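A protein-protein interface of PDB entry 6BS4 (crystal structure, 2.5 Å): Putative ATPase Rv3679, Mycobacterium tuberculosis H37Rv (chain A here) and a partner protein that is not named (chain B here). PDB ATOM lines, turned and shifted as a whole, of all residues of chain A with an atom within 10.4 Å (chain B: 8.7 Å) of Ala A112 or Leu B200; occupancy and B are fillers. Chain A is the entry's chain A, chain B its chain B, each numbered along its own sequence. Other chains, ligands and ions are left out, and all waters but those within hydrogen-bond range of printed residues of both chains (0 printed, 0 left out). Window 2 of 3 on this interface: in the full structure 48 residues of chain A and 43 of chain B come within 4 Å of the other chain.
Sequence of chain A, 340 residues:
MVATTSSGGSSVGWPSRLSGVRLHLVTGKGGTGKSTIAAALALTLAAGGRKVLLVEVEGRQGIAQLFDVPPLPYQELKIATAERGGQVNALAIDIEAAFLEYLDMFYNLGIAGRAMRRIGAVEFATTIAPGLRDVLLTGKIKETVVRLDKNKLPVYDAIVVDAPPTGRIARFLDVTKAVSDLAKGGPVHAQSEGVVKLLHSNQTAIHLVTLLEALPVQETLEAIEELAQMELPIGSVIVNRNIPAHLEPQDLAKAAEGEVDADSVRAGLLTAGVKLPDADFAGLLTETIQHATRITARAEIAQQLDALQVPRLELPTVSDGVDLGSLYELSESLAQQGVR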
ATOM      1  N   GLU A  96      -6.525  11.352  29.065  1.00  0.00           N
ATOM      2  CA  GLU A  96      -5.808  12.485  28.470  1.00  0.00           C
ATOM      3  C   GLU A  96      -4.405  12.069  28.037  1.00  0.00           C
ATOM      4  O   GLU A  96      -4.067  12.205  26.858  1.00  0.00           O
ATOM      5  CB  GLU A  96      -5.809  13.671  29.440  1.00  0.00           C
ATOM      6  CG  GLU A  96      -4.857  14.811  29.110  1.00  0.00           C
ATOM      7  CD  GLU A  96      -5.397  16.187  29.458  1.00  0.00           C
ATOM      8  OE1 GLU A  96      -4.835  17.174  28.941  1.00  0.00           O
ATOM      9  OE2 GLU A  96      -6.381  16.286  30.226  1.00  0.00           O
ATOM     10  N   PHE A  99      -4.583   9.639  25.183  1.00  0.00           N
ATOM     11  CA  PHE A  99      -4.876  10.299  23.904  1.00  0.00           C
ATOM     12  C   PHE A  99      -3.613  10.884  23.269  1.00  0.00           C
ATOM     13  O   PHE A  99      -3.417  10.703  22.068  1.00  0.00           O
ATOM     14  CB  PHE A  99      -6.027  11.340  24.017  1.00  0.00           C
ATOM     15  CG  PHE A  99      -6.423  12.038  22.726  1.00  0.00           C
ATOM     16  CD1 PHE A  99      -6.674  11.310  21.565  1.00  0.00           C
ATOM     17  CD2 PHE A  99      -6.540  13.421  22.670  1.00  0.00           C
ATOM     18  CE1 PHE A  99      -7.021  11.959  20.368  1.00  0.00           C
ATOM     19  CE2 PHE A  99      -6.907  14.067  21.481  1.00  0.00           C
ATOM     20  CZ  PHE A  99      -7.140  13.334  20.337  1.00  0.00           C
ATOM     21  N   LEU A 100      -2.744  11.539  24.081  1.00  0.00           N
ATOM     22  CA  LEU A 100      -1.455  12.110  23.655  1.00  0.00           C
ATOM     23  C   LEU A 100      -0.510  11.001  23.203  1.00  0.00           C
ATOM     24  O   LEU A 100       0.179  11.149  22.191  1.00  0.00           O
ATOM     25  CB  LEU A 100      -0.770  12.913  24.784  1.00  0.00           C
ATOM     26  CG  LEU A 100      -1.525  14.045  25.489  1.00  0.00           C
ATOM     27  CD1 LEU A 100      -0.587  14.811  26.405  1.00  0.00           C
ATOM     28  CD2 LEU A 100      -2.152  15.002  24.511  1.00  0.00           C
ATOM     29  N   GLU A 101      -0.468   9.905  23.964  1.00  0.00           N
ATOM     30  CA  GLU A 101       0.314   8.699  23.691  1.00  0.00           C
ATOM     31  C   GLU A 101      -0.091   8.155  22.303  1.00  0.00           C
ATOM     32  O   GLU A 101       0.771   7.819  21.491  1.00  0.00           O
ATOM     33  CB  GLU A 101      -0.031   7.669  24.777  1.00  0.00           C
ATOM     34  CG  GLU A 101       1.083   6.778  25.287  1.00  0.00           C
ATOM     35  CD  GLU A 101       0.691   6.007  26.537  1.00  0.00           C
ATOM     36  OE1 GLU A 101      -0.438   5.454  26.592  1.00  0.00           O
ATOM     37  OE2 GLU A 101       1.522   5.965  27.472  1.00  0.00           O
ATOM     38  N   TYR A 102      -1.414   8.106  22.039  1.00  0.00           N
ATOM     39  CA  TYR A 102      -2.027   7.651  20.792  1.00  0.00           C
ATOM     40  C   TYR A 102      -1.679   8.609  19.644  1.00  0.00           C
ATOM     41  O   TYR A 102      -1.291   8.136  18.577  1.00  0.00           O
ATOM     42  CB  TYR A 102      -3.540   7.539  21.010  1.00  0.00           C
ATOM     43  CG  TYR A 102      -4.399   7.329  19.785  1.00  0.00           C
ATOM     44  CD1 TYR A 102      -4.820   6.056  19.419  1.00  0.00           C
ATOM     45  CD2 TYR A 102      -4.937   8.414  19.096  1.00  0.00           C
ATOM     46  CE1 TYR A 102      -5.684   5.860  18.342  1.00  0.00           C
ATOM     47  CE2 TYR A 102      -5.788   8.233  18.007  1.00  0.00           C
ATOM     48  CZ  TYR A 102      -6.159   6.952  17.633  1.00  0.00           C
ATOM     49  OH  TYR A 102      -6.994   6.757  16.559  1.00  0.00           O
ATOM     50  N   LEU A 103      -1.805   9.945  19.862  1.00  0.00           N
ATOM     51  CA  LEU A 103      -1.474  10.981  18.876  1.00  0.00           C
ATOM     52  C   LEU A 103      -0.014  10.892  18.430  1.00  0.00           C
ATOM     53  O   LEU A 103       0.276  11.003  17.239  1.00  0.00           O
ATOM     54  CB  LEU A 103      -1.748  12.386  19.438  1.00  0.00           C
ATOM     55  CG  LEU A 103      -3.175  12.889  19.339  1.00  0.00           C
ATOM     56  CD1 LEU A 103      -3.378  14.063  20.247  1.00  0.00           C
ATOM     57  CD2 LEU A 103      -3.524  13.278  17.926  1.00  0.00           C
ATOM     58  N   ASP A 104       0.887  10.663  19.396  1.00  0.00           N
ATOM     59  CA  ASP A 104       2.326  10.529  19.200  1.00  0.00           C
ATOM     60  C   ASP A 104       2.724   9.224  18.495  1.00  0.00           C
ATOM     61  O   ASP A 104       3.514   9.278  17.556  1.00  0.00           O
ATOM     62  CB  ASP A 104       3.052  10.676  20.552  1.00  0.00           C
ATOM     63  CG  ASP A 104       4.566  10.637  20.498  1.00  0.00           C
ATOM     64  OD1 ASP A 104       5.152  11.298  19.598  1.00  0.00           O
ATOM     65  OD2 ASP A 104       5.171   9.966  21.366  1.00  0.00           O
ATOM     66  N   TYR A 107       0.169   8.954  14.895  1.00  0.00           N
ATOM     67  CA  TYR A 107       0.110  10.082  13.965  1.00  0.00           C
ATOM     68  C   TYR A 107       1.305  11.032  14.067  1.00  0.00           C
ATOM     69  O   TYR A 107       1.386  11.986  13.281  1.00  0.00           O
ATOM     70  CB  TYR A 107      -1.197  10.868  14.161  1.00  0.00           C
ATOM     71  CG  TYR A 107      -2.464  10.085  13.900  1.00  0.00           C
ATOM     72  CD1 TYR A 107      -3.012  10.013  12.623  1.00  0.00           C
ATOM     73  CD2 TYR A 107      -3.142   9.454  14.937  1.00  0.00           C
ATOM     74  CE1 TYR A 107      -4.204   9.329  12.382  1.00  0.00           C
ATOM     75  CE2 TYR A 107      -4.321   8.745  14.705  1.00  0.00           C
ATOM     76  CZ  TYR A 107      -4.856   8.696  13.427  1.00  0.00           C
ATOM     77  OH  TYR A 107      -6.025   8.010  13.195  1.00  0.00           O
ATOM     78  N   ASN A 108       2.226  10.778  15.028  1.00  0.00           N
ATOM     79  CA  ASN A 108       3.391  11.622  15.327  1.00  0.00           C
ATOM     80  C   ASN A 108       2.948  13.096  15.544  1.00  0.00           C
ATOM     81  O   ASN A 108       3.501  14.042  14.958  1.00  0.00           O
ATOM     82  CB  ASN A 108       4.524  11.443  14.287  1.00  0.00           C
ATOM     83  CG  ASN A 108       5.842  12.080  14.676  1.00  0.00           C
ATOM     84  OD1 ASN A 108       6.374  11.882  15.781  1.00  0.00           O
ATOM     85  ND2 ASN A 108       6.399  12.861  13.761  1.00  0.00           N
ATOM     86  N   LEU A 109       1.891  13.253  16.367  1.00  0.00           N
ATOM     87  CA  LEU A 109       1.277  14.534  16.712  1.00  0.00           C
ATOM     88  C   LEU A 109       1.476  14.912  18.186  1.00  0.00           C
ATOM     89  O   LEU A 109       0.645  15.617  18.760  1.00  0.00           O
ATOM     90  CB  LEU A 109      -0.219  14.570  16.309  1.00  0.00           C
ATOM     91  CG  LEU A 109      -0.540  14.726  14.817  1.00  0.00           C
ATOM     92  CD1 LEU A 109      -2.017  14.467  14.547  1.00  0.00           C
ATOM     93  CD2 LEU A 109      -0.139  16.115  14.294  1.00  0.00           C
ATOM     94  N   GLY A 110       2.603  14.477  18.761  1.00  0.00           N
ATOM     95  CA  GLY A 110       3.001  14.785  20.131  1.00  0.00           C
ATOM     96  C   GLY A 110       3.086  16.276  20.406  1.00  0.00           C
ATOM     97  O   GLY A 110       2.702  16.723  21.489  1.00  0.00           O
ATOM     98  N   ILE A 111       3.568  17.061  19.417  1.00  0.00           N
ATOM     99  CA  ILE A 111       3.674  18.529  19.497  1.00  0.00           C
ATOM    100  C   ILE A 111       2.286  19.170  19.644  1.00  0.00           C
ATOM    101  O   ILE A 111       2.062  19.944  20.576  1.00  0.00           O
ATOM    102  CB  ILE A 111       4.510  19.146  18.319  1.00  0.00           C
ATOM    103  CG1 ILE A 111       4.582  20.689  18.398  1.00  0.00           C
ATOM    104  CG2 ILE A 111       4.005  18.690  16.934  1.00  0.00           C
ATOM    105  CD1 ILE A 111       5.406  21.241  19.552  1.00  0.00           C
ATOM    106  N   ALA A 112       1.367  18.821  18.716  1.00  0.00           N
ATOM    107  CA  ALA A 112      -0.022  19.255  18.653  1.00  0.00           C
ATOM    108  C   ALA A 112      -0.742  18.829  19.931  1.00  0.00           C
ATOM    109  O   ALA A 112      -1.483  19.632  20.484  1.00  0.00           O
ATOM    110  CB  ALA A 112      -0.707  18.655  17.427  1.00  0.00           C
ATOM    111  N   GLY A 113      -0.456  17.616  20.410  1.00  0.00           N
ATOM    112  CA  GLY A 113      -1.019  17.055  21.631  1.00  0.00           C
ATOM    113  C   GLY A 113      -0.695  17.832  22.894  1.00  0.00           C
ATOM    114  O   GLY A 113      -1.589  18.093  23.703  1.00  0.00           O
ATOM    115  N   ARG A 114       0.586  18.205  23.075  1.00  0.00           N
ATOM    116  CA  ARG A 114       1.077  18.979  24.223  1.00  0.00           C
ATOM    117  C   ARG A 114       0.540  20.410  24.214  1.00  0.00           C
ATOM    118  O   ARG A 114       0.409  21.020  25.283  1.00  0.00           O
ATOM    119  CB  ARG A 114       2.614  18.956  24.291  1.00  0.00           C
ATOM    120  CG  ARG A 114       3.150  17.747  25.037  1.00  0.00           C
ATOM    121  CD  ARG A 114       4.662  17.644  24.936  1.00  0.00           C
ATOM    122  NE  ARG A 114       5.066  16.481  24.141  1.00  0.00           N
ATOM    123  CZ  ARG A 114       5.495  16.543  22.884  1.00  0.00           C
ATOM    124  NH1 ARG A 114       5.596  17.713  22.266  1.00  0.00           N
ATOM    125  NH2 ARG A 114       5.823  15.433  22.233  1.00  0.00           N
ATOM    126  N   ALA A 115       0.216  20.936  23.011  1.00  0.00           N
ATOM    127  CA  ALA A 115      -0.384  22.256  22.827  1.00  0.00           C
ATOM    128  C   ALA A 115      -1.852  22.187  23.274  1.00  0.00           C
ATOM    129  O   ALA A 115      -2.329  23.098  23.948  1.00  0.00           O
ATOM    130  CB  ALA A 115      -0.298  22.672  21.368  1.00  0.00           C
ATOM    131  N   MET A 116      -2.541  21.077  22.931  1.00  0.00           N
ATOM    132  CA  MET A 116      -3.941  20.797  23.263  1.00  0.00           C
ATOM    133  C   MET A 116      -4.182  20.681  24.777  1.00  0.00           C
ATOM    134  O   MET A 116      -5.189  21.187  25.281  1.00  0.00           O
ATOM    135  CB  MET A 116      -4.397  19.505  22.584  1.00  0.00           C
ATOM    136  CG  MET A 116      -4.583  19.634  21.106  1.00  0.00           C
ATOM    137  SD  MET A 116      -5.026  18.059  20.356  1.00  0.00           S
ATOM    138  CE  MET A 116      -6.828  18.073  20.594  1.00  0.00           C
ATOM    139  N   ARG A 117      -3.271  19.982  25.483  1.00  0.00           N
ATOM    140  CA  ARG A 117      -3.298  19.776  26.934  1.00  0.00           C
ATOM    141  C   ARG A 117      -3.302  21.159  27.634  1.00  0.00           C
ATOM    142  O   ARG A 117      -4.120  21.394  28.527  1.00  0.00           O
ATOM    143  CB  ARG A 117      -2.089  18.907  27.356  1.00  0.00           C
ATOM    144  CG  ARG A 117      -2.012  18.529  28.843  1.00  0.00           C
ATOM    145  CD  ARG A 117      -0.712  17.830  29.224  1.00  0.00           C
ATOM    146  NE  ARG A 117       0.438  18.699  28.975  1.00  0.00           N
ATOM    147  CZ  ARG A 117       1.662  18.272  28.686  1.00  0.00           C
ATOM    148  NH1 ARG A 117       1.928  16.971  28.645  1.00  0.00           N
ATOM    149  NH2 ARG A 117       2.633  19.142  28.446  1.00  0.00           N
ATOM    150  N   ARG A 118      -2.467  22.095  27.128  1.00  0.00           N
ATOM    151  CA  ARG A 118      -2.325  23.460  27.645  1.00  0.00           C
ATOM    152  C   ARG A 118      -3.581  24.336  27.487  1.00  0.00           C
ATOM    153  O   ARG A 118      -3.651  25.376  28.135  1.00  0.00           O
ATOM    154  CB  ARG A 118      -1.092  24.166  27.037  1.00  0.00           C
ATOM    155  CG  ARG A 118       0.242  23.589  27.494  1.00  0.00           C
ATOM    156  CD  ARG A 118       1.417  24.299  26.847  1.00  0.00           C
ATOM    157  NE  ARG A 118       2.580  23.414  26.727  1.00  0.00           N
ATOM    158  CZ  ARG A 118       3.155  23.070  25.576  1.00  0.00           C
ATOM    159  NH1 ARG A 118       2.696  23.550  24.425  1.00  0.00           N
ATOM    160  NH2 ARG A 118       4.203  22.256  25.568  1.00  0.00           N
ATOM    161  N   ILE A 119      -4.549  23.937  26.637  1.00  0.00           N
ATOM    162  CA  ILE A 119      -5.792  24.697  26.399  1.00  0.00           C
ATOM    163  C   ILE A 119      -7.074  23.885  26.750  1.00  0.00           C
ATOM    164  O   ILE A 119      -8.184  24.361  26.482  1.00  0.00           O
ATOM    165  CB  ILE A 119      -5.868  25.314  24.955  1.00  0.00           C
ATOM    166  CG1 ILE A 119      -5.910  24.231  23.857  1.00  0.00           C
ATOM    167  CG2 ILE A 119      -4.754  26.344  24.696  1.00  0.00           C
ATOM    168  CD1 ILE A 119      -6.728  24.588  22.666  1.00  0.00           C
ATOM    169  N   GLY A 120      -6.899  22.685  27.324  1.00  0.00           N
ATOM    170  CA  GLY A 120      -7.982  21.784  27.711  1.00  0.00           C
ATOM    171  C   GLY A 120      -8.678  21.088  26.555  1.00  0.00           C
ATOM    172  O   GLY A 120      -9.815  20.622  26.707  1.00  0.00           O
ATOM    173  N   ALA A 121      -7.993  20.980  25.402  1.00  0.00           N
ATOM    174  CA  ALA A 121      -8.547  20.421  24.166  1.00  0.00           C
ATOM    175  C   ALA A 121      -8.589  18.894  24.106  1.00  0.00           C
ATOM    176  O   ALA A 121      -9.337  18.343  23.292  1.00  0.00           O
ATOM    177  CB  ALA A 121      -7.800  20.984  22.958  1.00  0.00           C
ATOM    178  N   VAL A 122      -7.789  18.218  24.950  1.00  0.00           N
ATOM    179  CA  VAL A 122      -7.726  16.750  25.037  1.00  0.00           C
ATOM    180  C   VAL A 122      -8.976  16.301  25.802  1.00  0.00           C
ATOM    181  O   VAL A 122      -9.650  15.349  25.389  1.00  0.00           O
ATOM    182  CB  VAL A 122      -6.405  16.256  25.699  1.00  0.00           C
ATOM    183  CG1 VAL A 122      -6.292  14.737  25.665  1.00  0.00           C
ATOM    184  CG2 VAL A 122      -5.188  16.894  25.044  1.00  0.00           C
ATOM    185  N   ALA A 125     -12.052  16.860  23.333  1.00  0.00           N
ATOM    186  CA  ALA A 125     -12.022  15.767  22.349  1.00  0.00           C
ATOM    187  C   ALA A 125     -12.485  14.396  22.886  1.00  0.00           C
ATOM    188  O   ALA A 125     -13.227  13.696  22.195  1.00  0.00           O
ATOM    189  CB  ALA A 125     -10.628  15.643  21.767  1.00  0.00           C
ATOM    190  N   LEU B 183     -12.841  25.213  17.647  1.00  0.00           N
ATOM    191  CA  LEU B 183     -12.265  23.928  17.212  1.00  0.00           C
ATOM    192  C   LEU B 183     -13.128  23.145  16.201  1.00  0.00           C
ATOM    193  O   LEU B 183     -12.582  22.352  15.426  1.00  0.00           O
ATOM    194  CB  LEU B 183     -11.906  23.047  18.424  1.00  0.00           C
ATOM    195  CG  LEU B 183     -10.430  22.906  18.823  1.00  0.00           C
ATOM    196  CD1 LEU B 183      -9.758  24.250  19.040  1.00  0.00           C
ATOM    197  CD2 LEU B 183     -10.305  22.080  20.075  1.00  0.00           C
ATOM    198  N   ILE B 194      -7.057  28.211  11.963  1.00  0.00           N
ATOM    199  CA  ILE B 194      -6.859  29.658  11.875  1.00  0.00           C
ATOM    200  C   ILE B 194      -5.685  30.124  12.762  1.00  0.00           C
ATOM    201  O   ILE B 194      -4.711  30.674  12.232  1.00  0.00           O
ATOM    202  CB  ILE B 194      -8.160  30.491  12.107  1.00  0.00           C
ATOM    203  CG1 ILE B 194      -9.218  30.278  10.993  1.00  0.00           C
ATOM    204  CG2 ILE B 194      -7.826  31.975  12.267  1.00  0.00           C
ATOM    205  CD1 ILE B 194     -10.600  30.841  11.268  1.00  0.00           C
ATOM    206  N   THR B 195      -5.753  29.874  14.090  1.00  0.00           N
ATOM    207  CA  THR B 195      -4.699  30.257  15.047  1.00  0.00           C
ATOM    208  C   THR B 195      -3.489  29.298  14.913  1.00  0.00           C
ATOM    209  O   THR B 195      -3.434  28.496  13.979  1.00  0.00           O
ATOM    210  CB  THR B 195      -5.287  30.386  16.496  1.00  0.00           C
ATOM    211  OG1 THR B 195      -6.589  30.980  16.455  1.00  0.00           O
ATOM    212  CG2 THR B 195      -4.397  31.200  17.449  1.00  0.00           C
ATOM    213  N   GLY B 196      -2.515  29.441  15.809  1.00  0.00           N
ATOM    214  CA  GLY B 196      -1.336  28.590  15.889  1.00  0.00           C
ATOM    215  C   GLY B 196      -1.632  27.429  16.816  1.00  0.00           C
ATOM    216  O   GLY B 196      -1.404  26.272  16.452  1.00  0.00           O
ATOM    217  N   VAL B 197      -2.186  27.734  18.012  1.00  0.00           N
ATOM    218  CA  VAL B 197      -2.549  26.743  19.028  1.00  0.00           C
ATOM    219  C   VAL B 197      -3.900  26.123  18.678  1.00  0.00           C
ATOM    220  O   VAL B 197      -4.001  24.893  18.649  1.00  0.00           O
ATOM    221  CB  VAL B 197      -2.501  27.302  20.476  1.00  0.00           C
ATOM    222  CG1 VAL B 197      -2.737  26.198  21.503  1.00  0.00           C
ATOM    223  CG2 VAL B 197      -1.171  28.000  20.751  1.00  0.00           C
ATOM    224  N   MET B 198      -4.923  26.966  18.377  1.00  0.00           N
ATOM    225  CA  MET B 198      -6.255  26.494  17.977  1.00  0.00           C
ATOM    226  C   MET B 198      -6.157  25.708  16.683  1.00  0.00           C
ATOM    227  O   MET B 198      -6.872  24.720  16.533  1.00  0.00           O
ATOM    228  CB  MET B 198      -7.290  27.635  17.826  1.00  0.00           C
ATOM    229  CG  MET B 198      -7.573  28.425  19.101  1.00  0.00           C
ATOM    230  SD  MET B 198      -7.802  27.420  20.584  1.00  0.00           S
ATOM    231  CE  MET B 198      -9.518  27.543  20.803  1.00  0.00           C
ATOM    232  N   GLY B 199      -5.255  26.137  15.791  1.00  0.00           N
ATOM    233  CA  GLY B 199      -4.977  25.491  14.514  1.00  0.00           C
ATOM    234  C   GLY B 199      -4.335  24.123  14.665  1.00  0.00           C
ATOM    235  O   GLY B 199      -4.691  23.197  13.929  1.00  0.00           O
ATOM    236  N   LEU B 200      -3.385  23.981  15.624  1.00  0.00           N
ATOM    237  CA  LEU B 200      -2.723  22.708  15.937  1.00  0.00           C
ATOM    238  C   LEU B 200      -3.743  21.718  16.525  1.00  0.00           C
ATOM    239  O   LEU B 200      -3.721  20.541  16.162  1.00  0.00           O
ATOM    240  CB  LEU B 200      -1.553  22.900  16.921  1.00  0.00           C
ATOM    241  CG  LEU B 200      -0.163  23.126  16.322  1.00  0.00           C
ATOM    242  CD1 LEU B 200       0.830  23.522  17.398  1.00  0.00           C
ATOM    243  CD2 LEU B 200       0.354  21.886  15.592  1.00  0.00           C
ATOM    244  N   ALA B 201      -4.643  22.211  17.412  1.00  0.00           N
ATOM    245  CA  ALA B 201      -5.716  21.430  18.040  1.00  0.00           C
ATOM    246  C   ALA B 201      -6.727  20.999  16.983  1.00  0.00           C
ATOM    247  O   ALA B 201      -7.098  19.827  16.941  1.00  0.00           O
ATOM    248  CB  ALA B 201      -6.408  22.248  19.123  1.00  0.00           C
ATOM    249  N   MET B 202      -7.127  21.939  16.100  1.00  0.00           N
ATOM    250  CA  MET B 202      -8.061  21.708  14.997  1.00  0.00           C
ATOM    251  C   MET B 202      -7.540  20.672  14.017  1.00  0.00           C
ATOM    252  O   MET B 202      -8.318  19.827  13.570  1.00  0.00           O
ATOM    253  CB  MET B 202      -8.309  22.999  14.229  1.00  0.00           C
ATOM    254  CG  MET B 202      -9.621  23.626  14.529  1.00  0.00           C
ATOM    255  SD  MET B 202      -9.865  25.035  13.435  1.00  0.00           S
ATOM    256  CE  MET B 202      -8.829  26.292  14.257  1.00  0.00           C
ATOM    257  N   LYS B 203      -6.239  20.766  13.653  1.00  0.00           N
ATOM    258  CA  LYS B 203      -5.593  19.848  12.717  1.00  0.00           C
ATOM    259  C   LYS B 203      -5.614  18.439  13.305  1.00  0.00           C
ATOM    260  O   LYS B 203      -6.052  17.520  12.619  1.00  0.00           O
ATOM    261  CB  LYS B 203      -4.169  20.314  12.366  1.00  0.00           C
ATOM    262  CG  LYS B 203      -3.714  19.883  10.978  1.00  0.00           C
ATOM    263  CD  LYS B 203      -2.408  20.556  10.557  1.00  0.00           C
ATOM    264  CE  LYS B 203      -1.958  20.097   9.189  1.00  0.00           C
ATOM    265  NZ  LYS B 203      -0.581  20.561   8.862  1.00  0.00           N
ATOM    266  N   ALA B 204      -5.244  18.295  14.602  1.00  0.00           N
ATOM    267  CA  ALA B 204      -5.251  17.026  15.349  1.00  0.00           C
ATOM    268  C   ALA B 204      -6.645  16.382  15.400  1.00  0.00           C
ATOM    269  O   ALA B 204      -6.741  15.163  15.275  1.00  0.00           O
ATOM    270  CB  ALA B 204      -4.723  17.238  16.757  1.00  0.00           C
ATOM    271  N   LEU B 205      -7.713  17.194  15.568  1.00  0.00           N
ATOM    272  CA  LEU B 205      -9.098  16.713  15.602  1.00  0.00           C
ATOM    273  C   LEU B 205      -9.597  16.230  14.238  1.00  0.00           C
ATOM    274  O   LEU B 205     -10.355  15.265  14.180  1.00  0.00           O
ATOM    275  CB  LEU B 205     -10.055  17.760  16.187  1.00  0.00           C
ATOM    276  CG  LEU B 205      -9.974  18.031  17.694  1.00  0.00           C
ATOM    277  CD1 LEU B 205     -11.208  18.757  18.176  1.00  0.00           C
ATOM    278  CD2 LEU B 205      -9.818  16.749  18.487  1.00  0.00           C
ATOM    279  N   SER B 206      -9.173  16.898  13.149  1.00  0.00           N
ATOM    280  CA  SER B 206      -9.517  16.553  11.765  1.00  0.00           C
ATOM    281  C   SER B 206      -8.853  15.232  11.373  1.00  0.00           C
ATOM    282  O   SER B 206      -9.464  14.426  10.670  1.00  0.00           O
ATOM    283  CB  SER B 206      -9.053  17.653  10.812  1.00  0.00           C
ATOM    284  OG  SER B 206      -9.749  18.869  11.026  1.00  0.00           O
ATOM    285  N   THR B 207      -7.605  15.025  11.854  1.00  0.00           N
ATOM    286  CA  THR B 207      -6.739  13.870  11.626  1.00  0.00           C
ATOM    287  C   THR B 207      -7.231  12.614  12.359  1.00  0.00           C
ATOM    288  O   THR B 207      -7.087  11.516  11.828  1.00  0.00           O
ATOM    289  CB  THR B 207      -5.269  14.234  12.020  1.00  0.00           C
ATOM    290  OG1 THR B 207      -4.853  15.441  11.365  1.00  0.00           O
ATOM    291  CG2 THR B 207      -4.261  13.139  11.679  1.00  0.00           C
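The backbone carbonyl oxygen (O) of Leu A103 sits at hydrogen-bond distance from the backbone NH (N) of Leu A109, 2.9 Å away.
The backbone carbonyl oxygen (O) of Met A116 lies within hydrogen-bond range of the backbone NH (N) of Ala A121.
O of Lys B203 lies within hydrogen-bond range of OG1 of Thr B207, 2.7 Å away.
Tyr A107 touches Thr B207.
CD1 of Leu A109 touches CG2 of Thr B207 (3.9 Å).
O of Leu B200 touches CB of Ala A112 (3.8 Å).
Val B197 touches Ala A115.
Met A116 touches Ala B201.
Ala B204 touches Met A116 (CB to SD, 3.7 Å).
CD2 of Leu B205 touches CE of Met A116 (3.9 Å).
CD1 of Ile A119 touches SD of Met B198, 3.7 Å away.
Ala A121 touches Leu B183 (CB to CD2, 3.97 Å).
Ala A125 touches Leu B205.
Tyr A102 touches none of the printed residues of chain B.
No residue of chain B comes within 4 Å of Gly A110.
Of chain B, only Leu B200 (3.8 Å) comes within 4 Å of Ala A112.
No residue of chain B comes within 4 Å of Gly A113.
Of the printed residues of chain B, Ala A121 touches Leu B183 (3.97 Å).
Of the printed residues of chain A, Leu B183 touches Ala A121 (3.97 Å).
No residue of chain A comes within 4 Å of Gly B196.
Of the printed residues of chain A, Met B198 touches Ile A119.
No residue of chain A comes within 4 Å of Gly B199.
Of chain A, only Met A116 comes within 4 Å of Ala B201.
Ala B204 touches just one residue of chain A: Met A116.
Of the printed residues of chain A, Thr B207 touches Tyr A107 and Leu A109.
The nearest residue of chain B that does not touch Ala A112 is Ala B204 (4.3 Å).
The nearest printed residue of chain B that does not touch Met A116 is Leu B200 (5.0 Å).
Of the 15 printed residues of chain B, 8 touch a printed residue of chain A.
Along chain B the printed residues that touch a printed residue of chain A span positions 183 to 207.
Of the 24 printed residues of chain A, 8 touch a printed residue of chain B.
Printed residues of chain A that touch a printed residue of chain B: Tyr A107, Leu A109, Ala A112, Ala A115, Met A116, Ile A119, Ala A121 and Ala A125.
Hydrophobic or aromatic side chains of chain A that line the printed part of chain B: Tyr A107, Leu A109, Ala A112, Met A116, Ile A119, Ala A121 and Ala A125.
Along chain A the printed residues that touch a printed residue of chain B span positions 107 to 125.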
